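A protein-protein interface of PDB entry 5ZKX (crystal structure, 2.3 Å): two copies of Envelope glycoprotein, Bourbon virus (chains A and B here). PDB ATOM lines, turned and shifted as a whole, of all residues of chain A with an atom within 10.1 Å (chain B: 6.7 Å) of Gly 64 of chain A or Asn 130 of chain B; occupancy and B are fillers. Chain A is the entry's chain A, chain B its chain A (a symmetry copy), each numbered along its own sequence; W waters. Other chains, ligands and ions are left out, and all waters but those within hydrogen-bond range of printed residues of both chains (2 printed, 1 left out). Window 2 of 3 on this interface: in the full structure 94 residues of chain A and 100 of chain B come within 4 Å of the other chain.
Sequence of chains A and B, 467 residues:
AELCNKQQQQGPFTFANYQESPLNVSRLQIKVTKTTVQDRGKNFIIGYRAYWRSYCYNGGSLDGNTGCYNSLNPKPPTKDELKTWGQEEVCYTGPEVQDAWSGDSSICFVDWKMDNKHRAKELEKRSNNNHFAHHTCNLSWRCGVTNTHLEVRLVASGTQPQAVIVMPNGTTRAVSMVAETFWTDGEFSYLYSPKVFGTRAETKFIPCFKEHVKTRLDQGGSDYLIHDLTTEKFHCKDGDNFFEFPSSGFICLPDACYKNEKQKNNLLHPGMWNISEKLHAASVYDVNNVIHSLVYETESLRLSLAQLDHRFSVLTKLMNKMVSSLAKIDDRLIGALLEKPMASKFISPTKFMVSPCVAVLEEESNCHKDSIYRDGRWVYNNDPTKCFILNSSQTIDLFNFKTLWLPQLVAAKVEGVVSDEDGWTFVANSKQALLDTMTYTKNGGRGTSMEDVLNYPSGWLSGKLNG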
ATOM      1  N   TYR A  57     -32.116 -21.865   5.877  1.00  0.00           N
ATOM      2  CA  TYR A  57     -31.574 -23.079   6.473  1.00  0.00           C
ATOM      3  C   TYR A  57     -30.114 -22.844   6.828  1.00  0.00           C
ATOM      4  O   TYR A  57     -29.352 -22.302   6.021  1.00  0.00           O
ATOM      5  CB  TYR A  57     -31.692 -24.284   5.532  1.00  0.00           C
ATOM      6  CG  TYR A  57     -31.147 -25.562   6.138  1.00  0.00           C
ATOM      7  CD1 TYR A  57     -31.799 -26.184   7.196  1.00  0.00           C
ATOM      8  CD2 TYR A  57     -29.975 -26.139   5.661  1.00  0.00           C
ATOM      9  CE1 TYR A  57     -31.304 -27.349   7.757  1.00  0.00           C
ATOM     10  CE2 TYR A  57     -29.471 -27.303   6.219  1.00  0.00           C
ATOM     11  CZ  TYR A  57     -30.139 -27.902   7.266  1.00  0.00           C
ATOM     12  OH  TYR A  57     -29.644 -29.060   7.821  1.00  0.00           O
ATOM     13  N   ASN A  58     -29.730 -23.240   8.037  1.00  0.00           N
ATOM     14  CA  ASN A  58     -28.352 -23.127   8.505  1.00  0.00           C
ATOM     15  C   ASN A  58     -27.823 -24.535   8.744  1.00  0.00           C
ATOM     16  O   ASN A  58     -28.103 -25.143   9.781  1.00  0.00           O
ATOM     17  CB  ASN A  58     -28.263 -22.282   9.770  1.00  0.00           C
ATOM     18  CG  ASN A  58     -26.843 -22.132  10.263  1.00  0.00           C
ATOM     19  OD1 ASN A  58     -25.893 -22.486   9.564  1.00  0.00           O
ATOM     20  ND2 ASN A  58     -26.687 -21.610  11.470  1.00  0.00           N
ATOM     21  N   GLY A  59     -27.066 -25.050   7.782  1.00  0.00           N
ATOM     22  CA  GLY A  59     -26.442 -26.348   7.925  1.00  0.00           C
ATOM     23  C   GLY A  59     -24.935 -26.238   7.855  1.00  0.00           C
ATOM     24  O   GLY A  59     -24.233 -27.239   7.682  1.00  0.00           O
ATOM     25  N   GLY A  60     -24.431 -25.014   7.984  1.00  0.00           N
ATOM     26  CA  GLY A  60     -23.012 -24.752   7.906  1.00  0.00           C
ATOM     27  C   GLY A  60     -22.547 -24.490   6.487  1.00  0.00           C
ATOM     28  O   GLY A  60     -23.235 -24.762   5.502  1.00  0.00           O
ATOM     29  N   SER A  61     -21.328 -23.955   6.391  1.00  0.00           N
ATOM     30  CA  SER A  61     -20.769 -23.542   5.109  1.00  0.00           C
ATOM     31  C   SER A  61     -20.506 -24.708   4.166  1.00  0.00           C
ATOM     32  O   SER A  61     -20.296 -24.477   2.971  1.00  0.00           O
ATOM     33  CB  SER A  61     -19.476 -22.762   5.338  1.00  0.00           C
ATOM     34  OG  SER A  61     -19.639 -21.817   6.381  1.00  0.00           O
ATOM     35  N   LEU A  62     -20.508 -25.942   4.667  1.00  0.00           N
ATOM     36  CA  LEU A  62     -20.279 -27.090   3.801  1.00  0.00           C
ATOM     37  C   LEU A  62     -21.553 -27.532   3.095  1.00  0.00           C
ATOM     38  O   LEU A  62     -21.488 -28.039   1.968  1.00  0.00           O
ATOM     39  CB  LEU A  62     -19.698 -28.253   4.609  1.00  0.00           C
ATOM     40  CG  LEU A  62     -18.266 -28.098   5.126  1.00  0.00           C
ATOM     41  CD1 LEU A  62     -17.949 -29.162   6.165  1.00  0.00           C
ATOM     42  CD2 LEU A  62     -17.270 -28.159   3.985  1.00  0.00           C
ATOM     43  N   ASP A  63     -22.707 -27.348   3.727  1.00  0.00           N
ATOM     44  CA  ASP A  63     -23.960 -27.787   3.131  1.00  0.00           C
ATOM     45  C   ASP A  63     -24.360 -26.853   1.996  1.00  0.00           C
ATOM     46  O   ASP A  63     -24.392 -25.631   2.163  1.00  0.00           O
ATOM     47  CB  ASP A  63     -25.060 -27.841   4.189  1.00  0.00           C
ATOM     48  CG  ASP A  63     -26.267 -28.630   3.729  1.00  0.00           C
ATOM     49  OD1 ASP A  63     -26.270 -29.084   2.568  1.00  0.00           O
ATOM     50  OD2 ASP A  63     -27.211 -28.796   4.524  1.00  0.00           O
ATOM     51  N   GLY A  64     -24.668 -27.433   0.835  1.00  0.00           N
ATOM     52  CA  GLY A  64     -25.133 -26.634  -0.283  1.00  0.00           C
ATOM     53  C   GLY A  64     -26.487 -25.995  -0.061  1.00  0.00           C
ATOM     54  O   GLY A  64     -26.798 -24.988  -0.705  1.00  0.00           O
ATOM     55  N   ASN A  65     -27.295 -26.551   0.838  1.00  0.00           N
ATOM     56  CA  ASN A  65     -28.610 -26.007   1.145  1.00  0.00           C
ATOM     57  C   ASN A  65     -28.567 -24.893   2.181  1.00  0.00           C
ATOM     58  O   ASN A  65     -29.626 -24.413   2.597  1.00  0.00           O
ATOM     59  CB  ASN A  65     -29.539 -27.122   1.626  1.00  0.00           C
ATOM     60  CG  ASN A  65     -29.648 -28.253   0.629  1.00  0.00           C
ATOM     61  OD1 ASN A  65     -29.371 -28.077  -0.558  1.00  0.00           O
ATOM     62  ND2 ASN A  65     -30.055 -29.424   1.104  1.00  0.00           N
ATOM     63  N   THR A  66     -27.381 -24.473   2.608  1.00  0.00           N
ATOM     64  CA  THR A  66     -27.264 -23.379   3.563  1.00  0.00           C
ATOM     65  C   THR A  66     -27.497 -22.052   2.849  1.00  0.00           C
ATOM     66  O   THR A  66     -26.823 -21.740   1.859  1.00  0.00           O
ATOM     67  CB  THR A  66     -25.895 -23.398   4.235  1.00  0.00           C
ATOM     68  OG1 THR A  66     -25.683 -24.675   4.849  1.00  0.00           O
ATOM     69  CG2 THR A  66     -25.821 -22.315   5.295  1.00  0.00           C
ATOM     70  N   GLY A  67     -28.439 -21.276   3.351  1.00  0.00           N
ATOM     71  CA  GLY A  67     -28.788 -20.012   2.735  1.00  0.00           C
ATOM     72  C   GLY A  67     -30.248 -19.693   2.978  1.00  0.00           C
ATOM     73  O   GLY A  67     -30.961 -20.409   3.678  1.00  0.00           O
ATOM     74  N   CYS A  68     -30.680 -18.591   2.372  1.00  0.00           N
ATOM     75  CA  CYS A  68     -32.024 -18.066   2.554  1.00  0.00           C
ATOM     76  C   CYS A  68     -32.765 -18.043   1.227  1.00  0.00           C
ATOM     77  O   CYS A  68     -32.199 -17.678   0.191  1.00  0.00           O
ATOM     78  CB  CYS A  68     -31.994 -16.656   3.144  1.00  0.00           C
ATOM     79  SG  CYS A  68     -31.544 -16.593   4.883  1.00  0.00           S
ATOM     80  N   TYR A  69     -34.029 -18.431   1.270  1.00  0.00           N
ATOM     81  CA  TYR A  69     -34.935 -18.312   0.137  1.00  0.00           C
ATOM     82  C   TYR A  69     -35.974 -17.263   0.529  1.00  0.00           C
ATOM     83  O   TYR A  69     -36.877 -17.537   1.325  1.00  0.00           O
ATOM     84  CB  TYR A  69     -35.570 -19.659  -0.206  1.00  0.00           C
ATOM     85  CG  TYR A  69     -34.662 -20.608  -0.967  1.00  0.00           C
ATOM     86  CD1 TYR A  69     -35.154 -21.374  -2.019  1.00  0.00           C
ATOM     87  CD2 TYR A  69     -33.318 -20.745  -0.634  1.00  0.00           C
ATOM     88  CE1 TYR A  69     -34.333 -22.246  -2.719  1.00  0.00           C
ATOM     89  CE2 TYR A  69     -32.490 -21.612  -1.327  1.00  0.00           C
ATOM     90  CZ  TYR A  69     -33.002 -22.361  -2.370  1.00  0.00           C
ATOM     91  OH  TYR A  69     -32.186 -23.228  -3.068  1.00  0.00           O
ATOM     92  N   ASN A 129     -30.878 -16.511  10.132  1.00  0.00           N
ATOM     93  CA  ASN A 129     -30.493 -17.886   9.818  1.00  0.00           C
ATOM     94  C   ASN A 129     -29.503 -18.403  10.861  1.00  0.00           C
ATOM     95  O   ASN A 129     -28.449 -18.953  10.538  1.00  0.00           O
ATOM     96  CB  ASN A 129     -29.910 -17.962   8.409  1.00  0.00           C
ATOM     97  CG  ASN A 129     -29.821 -19.378   7.891  1.00  0.00           C
ATOM     98  OD1 ASN A 129     -30.627 -20.234   8.248  1.00  0.00           O
ATOM     99  ND2 ASN A 129     -28.836 -19.632   7.042  1.00  0.00           N
ATOM    100  N   HIS A 135     -34.032 -25.101  10.017  1.00  0.00           N
ATOM    101  CA  HIS A 135     -34.660 -24.077   9.197  1.00  0.00           C
ATOM    102  C   HIS A 135     -35.188 -22.951  10.074  1.00  0.00           C
ATOM    103  O   HIS A 135     -35.504 -23.150  11.248  1.00  0.00           O
ATOM    104  CB  HIS A 135     -35.810 -24.659   8.377  1.00  0.00           C
ATOM    105  CG  HIS A 135     -35.369 -25.547   7.256  1.00  0.00           C
ATOM    106  ND1 HIS A 135     -35.024 -25.062   6.014  1.00  0.00           N
ATOM    107  CD2 HIS A 135     -35.224 -26.891   7.189  1.00  0.00           C
ATOM    108  CE1 HIS A 135     -34.682 -26.069   5.230  1.00  0.00           C
ATOM    109  NE2 HIS A 135     -34.794 -27.189   5.920  1.00  0.00           N
ATOM    110  N   CYS B  56     -19.072 -13.900  -5.201  1.00  0.00           N
ATOM    111  CA  CYS B  56     -18.944 -14.384  -3.838  1.00  0.00           C
ATOM    112  C   CYS B  56     -17.904 -15.493  -3.752  1.00  0.00           C
ATOM    113  O   CYS B  56     -17.600 -16.173  -4.735  1.00  0.00           O
ATOM    114  CB  CYS B  56     -20.293 -14.889  -3.317  1.00  0.00           C
ATOM    115  SG  CYS B  56     -21.640 -13.695  -3.467  1.00  0.00           S
ATOM    116  N   ASN B  58     -16.974 -18.725  -0.907  1.00  0.00           N
ATOM    117  CA  ASN B  58     -17.339 -19.481   0.289  1.00  0.00           C
ATOM    118  C   ASN B  58     -16.140 -20.332   0.686  1.00  0.00           C
ATOM    119  O   ASN B  58     -15.908 -21.398   0.109  1.00  0.00           O
ATOM    120  CB  ASN B  58     -18.571 -20.343   0.045  1.00  0.00           C
ATOM    121  CG  ASN B  58     -18.981 -21.119   1.276  1.00  0.00           C
ATOM    122  OD1 ASN B  58     -18.477 -20.876   2.372  1.00  0.00           O
ATOM    123  ND2 ASN B  58     -19.897 -22.061   1.103  1.00  0.00           N
ATOM    124  N   ASP B  99     -25.530 -18.695 -11.067  1.00  0.00           N
ATOM    125  CA  ASP B  99     -24.980 -19.864 -10.380  1.00  0.00           C
ATOM    126  C   ASP B  99     -23.769 -20.428 -11.116  1.00  0.00           C
ATOM    127  O   ASP B  99     -23.609 -21.644 -11.246  1.00  0.00           O
ATOM    128  CB  ASP B  99     -26.046 -20.946 -10.183  1.00  0.00           C
ATOM    129  CG  ASP B  99     -25.714 -21.883  -9.038  1.00  0.00           C
ATOM    130  OD1 ASP B  99     -26.586 -22.690  -8.655  1.00  0.00           O
ATOM    131  OD2 ASP B  99     -24.583 -21.809  -8.517  1.00  0.00           O
ATOM    132  N   ASN B 128     -25.764 -15.827  -4.564  1.00  0.00           N
ATOM    133  CA  ASN B 128     -25.679 -17.060  -3.794  1.00  0.00           C
ATOM    134  C   ASN B 128     -24.212 -17.396  -3.568  1.00  0.00           C
ATOM    135  O   ASN B 128     -23.373 -17.157  -4.439  1.00  0.00           O
ATOM    136  CB  ASN B 128     -26.400 -18.219  -4.493  1.00  0.00           C
ATOM    137  CG  ASN B 128     -25.719 -18.651  -5.769  1.00  0.00           C
ATOM    138  OD1 ASN B 128     -25.733 -17.936  -6.771  1.00  0.00           O
ATOM    139  ND2 ASN B 128     -25.122 -19.834  -5.745  1.00  0.00           N
ATOM    140  N   ASN B 129     -23.915 -17.935  -2.388  1.00  0.00           N
ATOM    141  CA  ASN B 129     -22.546 -18.240  -1.973  1.00  0.00           C
ATOM    142  C   ASN B 129     -22.491 -19.625  -1.330  1.00  0.00           C
ATOM    143  O   ASN B 129     -21.939 -19.815  -0.245  1.00  0.00           O
ATOM    144  CB  ASN B 129     -22.031 -17.162  -1.021  1.00  0.00           C
ATOM    145  CG  ASN B 129     -20.534 -17.218  -0.834  1.00  0.00           C
ATOM    146  OD1 ASN B 129     -19.799 -17.618  -1.734  1.00  0.00           O
ATOM    147  ND2 ASN B 129     -20.073 -16.815   0.340  1.00  0.00           N
ATOM    148  N   ASN B 130     -23.077 -20.619  -2.001  1.00  0.00           N
ATOM    149  CA  ASN B 130     -23.298 -21.937  -1.417  1.00  0.00           C
ATOM    150  C   ASN B 130     -22.391 -23.013  -2.014  1.00  0.00           C
ATOM    151  O   ASN B 130     -22.760 -24.190  -2.047  1.00  0.00           O
ATOM    152  CB  ASN B 130     -24.761 -22.341  -1.580  1.00  0.00           C
ATOM    153  CG  ASN B 130     -25.161 -22.477  -3.034  1.00  0.00           C
ATOM    154  OD1 ASN B 130     -24.712 -21.709  -3.884  1.00  0.00           O
ATOM    155  ND2 ASN B 130     -26.000 -23.461  -3.331  1.00  0.00           N
ATOM    156  N   HIS B 131     -21.209 -22.636  -2.491  1.00  0.00           N
ATOM    157  CA  HIS B 131     -20.247 -23.591  -3.036  1.00  0.00           C
ATOM    158  C   HIS B 131     -18.959 -23.452  -2.234  1.00  0.00           C
ATOM    159  O   HIS B 131     -18.189 -22.508  -2.440  1.00  0.00           O
ATOM    160  CB  HIS B 131     -20.025 -23.357  -4.527  1.00  0.00           C
ATOM    161  CG  HIS B 131     -21.241 -23.616  -5.358  1.00  0.00           C
ATOM    162  ND1 HIS B 131     -21.718 -24.887  -5.602  1.00  0.00           N
ATOM    163  CD2 HIS B 131     -22.091 -22.769  -5.987  1.00  0.00           C
ATOM    164  CE1 HIS B 131     -22.803 -24.811  -6.353  1.00  0.00           C
ATOM    165  NE2 HIS B 131     -23.050 -23.537  -6.599  1.00  0.00           N
ATOM    166  N   PHE B 132     -18.731 -24.394  -1.322  1.00  0.00           N
ATOM    167  CA  PHE B 132     -17.640 -24.260  -0.369  1.00  0.00           C
ATOM    168  C   PHE B 132     -16.286 -24.398  -1.055  1.00  0.00           C
ATOM    169  O   PHE B 132     -16.120 -25.193  -1.984  1.00  0.00           O
ATOM    170  CB  PHE B 132     -17.769 -25.296   0.742  1.00  0.00           C
ATOM    171  CG  PHE B 132     -16.778 -25.108   1.846  1.00  0.00           C
ATOM    172  CD1 PHE B 132     -16.968 -24.126   2.801  1.00  0.00           C
ATOM    173  CD2 PHE B 132     -15.644 -25.895   1.917  1.00  0.00           C
ATOM    174  CE1 PHE B 132     -16.054 -23.942   3.815  1.00  0.00           C
ATOM    175  CE2 PHE B 132     -14.725 -25.717   2.929  1.00  0.00           C
ATOM    176  CZ  PHE B 132     -14.930 -24.736   3.879  1.00  0.00           C
ATOM    177  N   THR B 136     -18.470 -17.994  -6.602  1.00  0.00           N
ATOM    178  CA  THR B 136     -19.748 -18.039  -7.299  1.00  0.00           C
ATOM    179  C   THR B 136     -19.974 -16.710  -8.006  1.00  0.00           C
ATOM    180  O   THR B 136     -19.618 -15.651  -7.483  1.00  0.00           O
ATOM    181  CB  THR B 136     -20.914 -18.329  -6.341  1.00  0.00           C
ATOM    182  OG1 THR B 136     -20.599 -19.473  -5.539  1.00  0.00           O
ATOM    183  CG2 THR B 136     -22.195 -18.612  -7.124  1.00  0.00           C
ATOM    184  N   ASN B 443     -32.196 -15.803  -4.444  1.00  0.00           N
ATOM    185  CA  ASN B 443     -31.184 -16.845  -4.351  1.00  0.00           C
ATOM    186  C   ASN B 443     -30.972 -17.471  -5.722  1.00  0.00           C
ATOM    187  O   ASN B 443     -31.906 -18.028  -6.308  1.00  0.00           O
ATOM    188  CB  ASN B 443     -31.589 -17.906  -3.331  1.00  0.00           C
ATOM    189  CG  ASN B 443     -30.391 -18.595  -2.706  1.00  0.00           C
ATOM    190  OD1 ASN B 443     -29.642 -19.297  -3.385  1.00  0.00           O
ATOM    191  ND2 ASN B 443     -30.198 -18.387  -1.410  1.00  0.00           N
ATOM    192  N   GLY B 444     -29.746 -17.380  -6.233  1.00  0.00           N
ATOM    193  CA  GLY B 444     -29.419 -17.969  -7.515  1.00  0.00           C
ATOM    194  C   GLY B 444     -29.117 -19.452  -7.446  1.00  0.00           C
ATOM    195  O   GLY B 444     -28.545 -20.016  -8.384  1.00  0.00           O
ATOM    196  N   GLY B 445     -29.497 -20.096  -6.344  1.00  0.00           N
ATOM    197  CA  GLY B 445     -29.262 -21.515  -6.158  1.00  0.00           C
ATOM    198  C   GLY B 445     -30.105 -22.388  -7.061  1.00  0.00           C
ATOM    199  O   GLY B 445     -31.275 -22.647  -6.774  1.00  0.00           O
HETATM  200  O   HOH W   1     -19.184 -19.409   4.363  1.00  0.00           O
HETATM  201  O   HOH W   2     -33.355 -14.851  -1.350  1.00  0.00           O
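The side-chain amide nitrogen (ND2) of Asn 58 of chain B is in hydrogen-bond range of the backbone carbonyl oxygen (O) of Ser 61 of chain A, 3.1 Å away.
The side-chain amide nitrogen of Asn 130 of chain B sits at hydrogen-bond distance from the backbone carbonyl oxygen of Gly 64 of chain A.
O of Cys 68 of chain A lies within hydrogen-bond range of ND2 of Asn 443 of chain B.
The backbone NH of Asn 58 of chain B sits at hydrogen-bond distance from the side-chain amide oxygen of Asn 129 of chain B (3.1 Å).
The side-chain amide oxygen of Asn 130 of chain B lies within hydrogen-bond range of the side-chain amide nitrogen of Asn 128 of chain B (2.7 Å).
The side-chain amide oxygen (OD1) of Asn 443 of chain B is in hydrogen-bond range of the backbone NH (N) of Gly 445 of chain B (3.1 Å).
O of Ser 61 of chain A touches CD1 of Phe 132 of chain B (3.4 Å).
Leu 62 of chain A touches Phe 132 of chain B (CD2 to CD2, 3.5 Å).
Tyr 69 of chain A touches Asn 443 of chain B (CE2 to CG, 3.9 Å).
O of Gly 445 of chain B touches OH of Tyr 69 of chain A, at 3.9 Å.
Of chain B, only Asn 130 (3.1 Å) comes within 4 Å of Gly 64 of chain A.
Asn 65 of chain A touches none of the printed residues of chain B.
Of the printed residues of chain B, Cys 68 of chain A touches Asn 443.
Printed residues of chain B within 4 Å of Tyr 69 of chain A: Asn 443 and Gly 445.
No residue of chain A comes within 4 Å of Asn 129 of chain B.
Of chain A, only Gly 64 comes within 4 Å of Asn 130 of chain B.
No residue of chain A comes within 4 Å of His 131 of chain B.
The nearest printed residue of chain A that does not touch Phe 132 of chain B is Asp 63 of chain A (6.1 Å).
Of the 12 printed residues of chain B, 5 touch a printed residue of chain A.
Hydrophobic or aromatic side chains of chain B that line the printed part of chain A: Phe 132.
Printed residues of chain A that touch a printed residue of chain B: Ser 61, Leu 62, Gly 64, Cys 68 and Tyr 69.
Hydrophobic or aromatic side chains of chain A within 4 Å of the printed part of chain B: Leu 62 and Tyr 69.
Among the printed residues, 7 pairs touch across the chains.
Among the printed residues, no Asp or Glu carboxylate lies within 4 Å of a Lys or Arg side-chain nitrogen of the other chain.
Positions printed for both chains: 58 and 129.
Water W1 bridges OD1 of Asn 58 of chain B (2.6 Å) and OG of Ser 61 of chain A (3.2 Å).
Water W2 bridges the backbone carbonyl oxygen of Cys 68 of chain A (3.4 Å) and the backbone NH of Asn 443 of chain B (3.4 Å).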
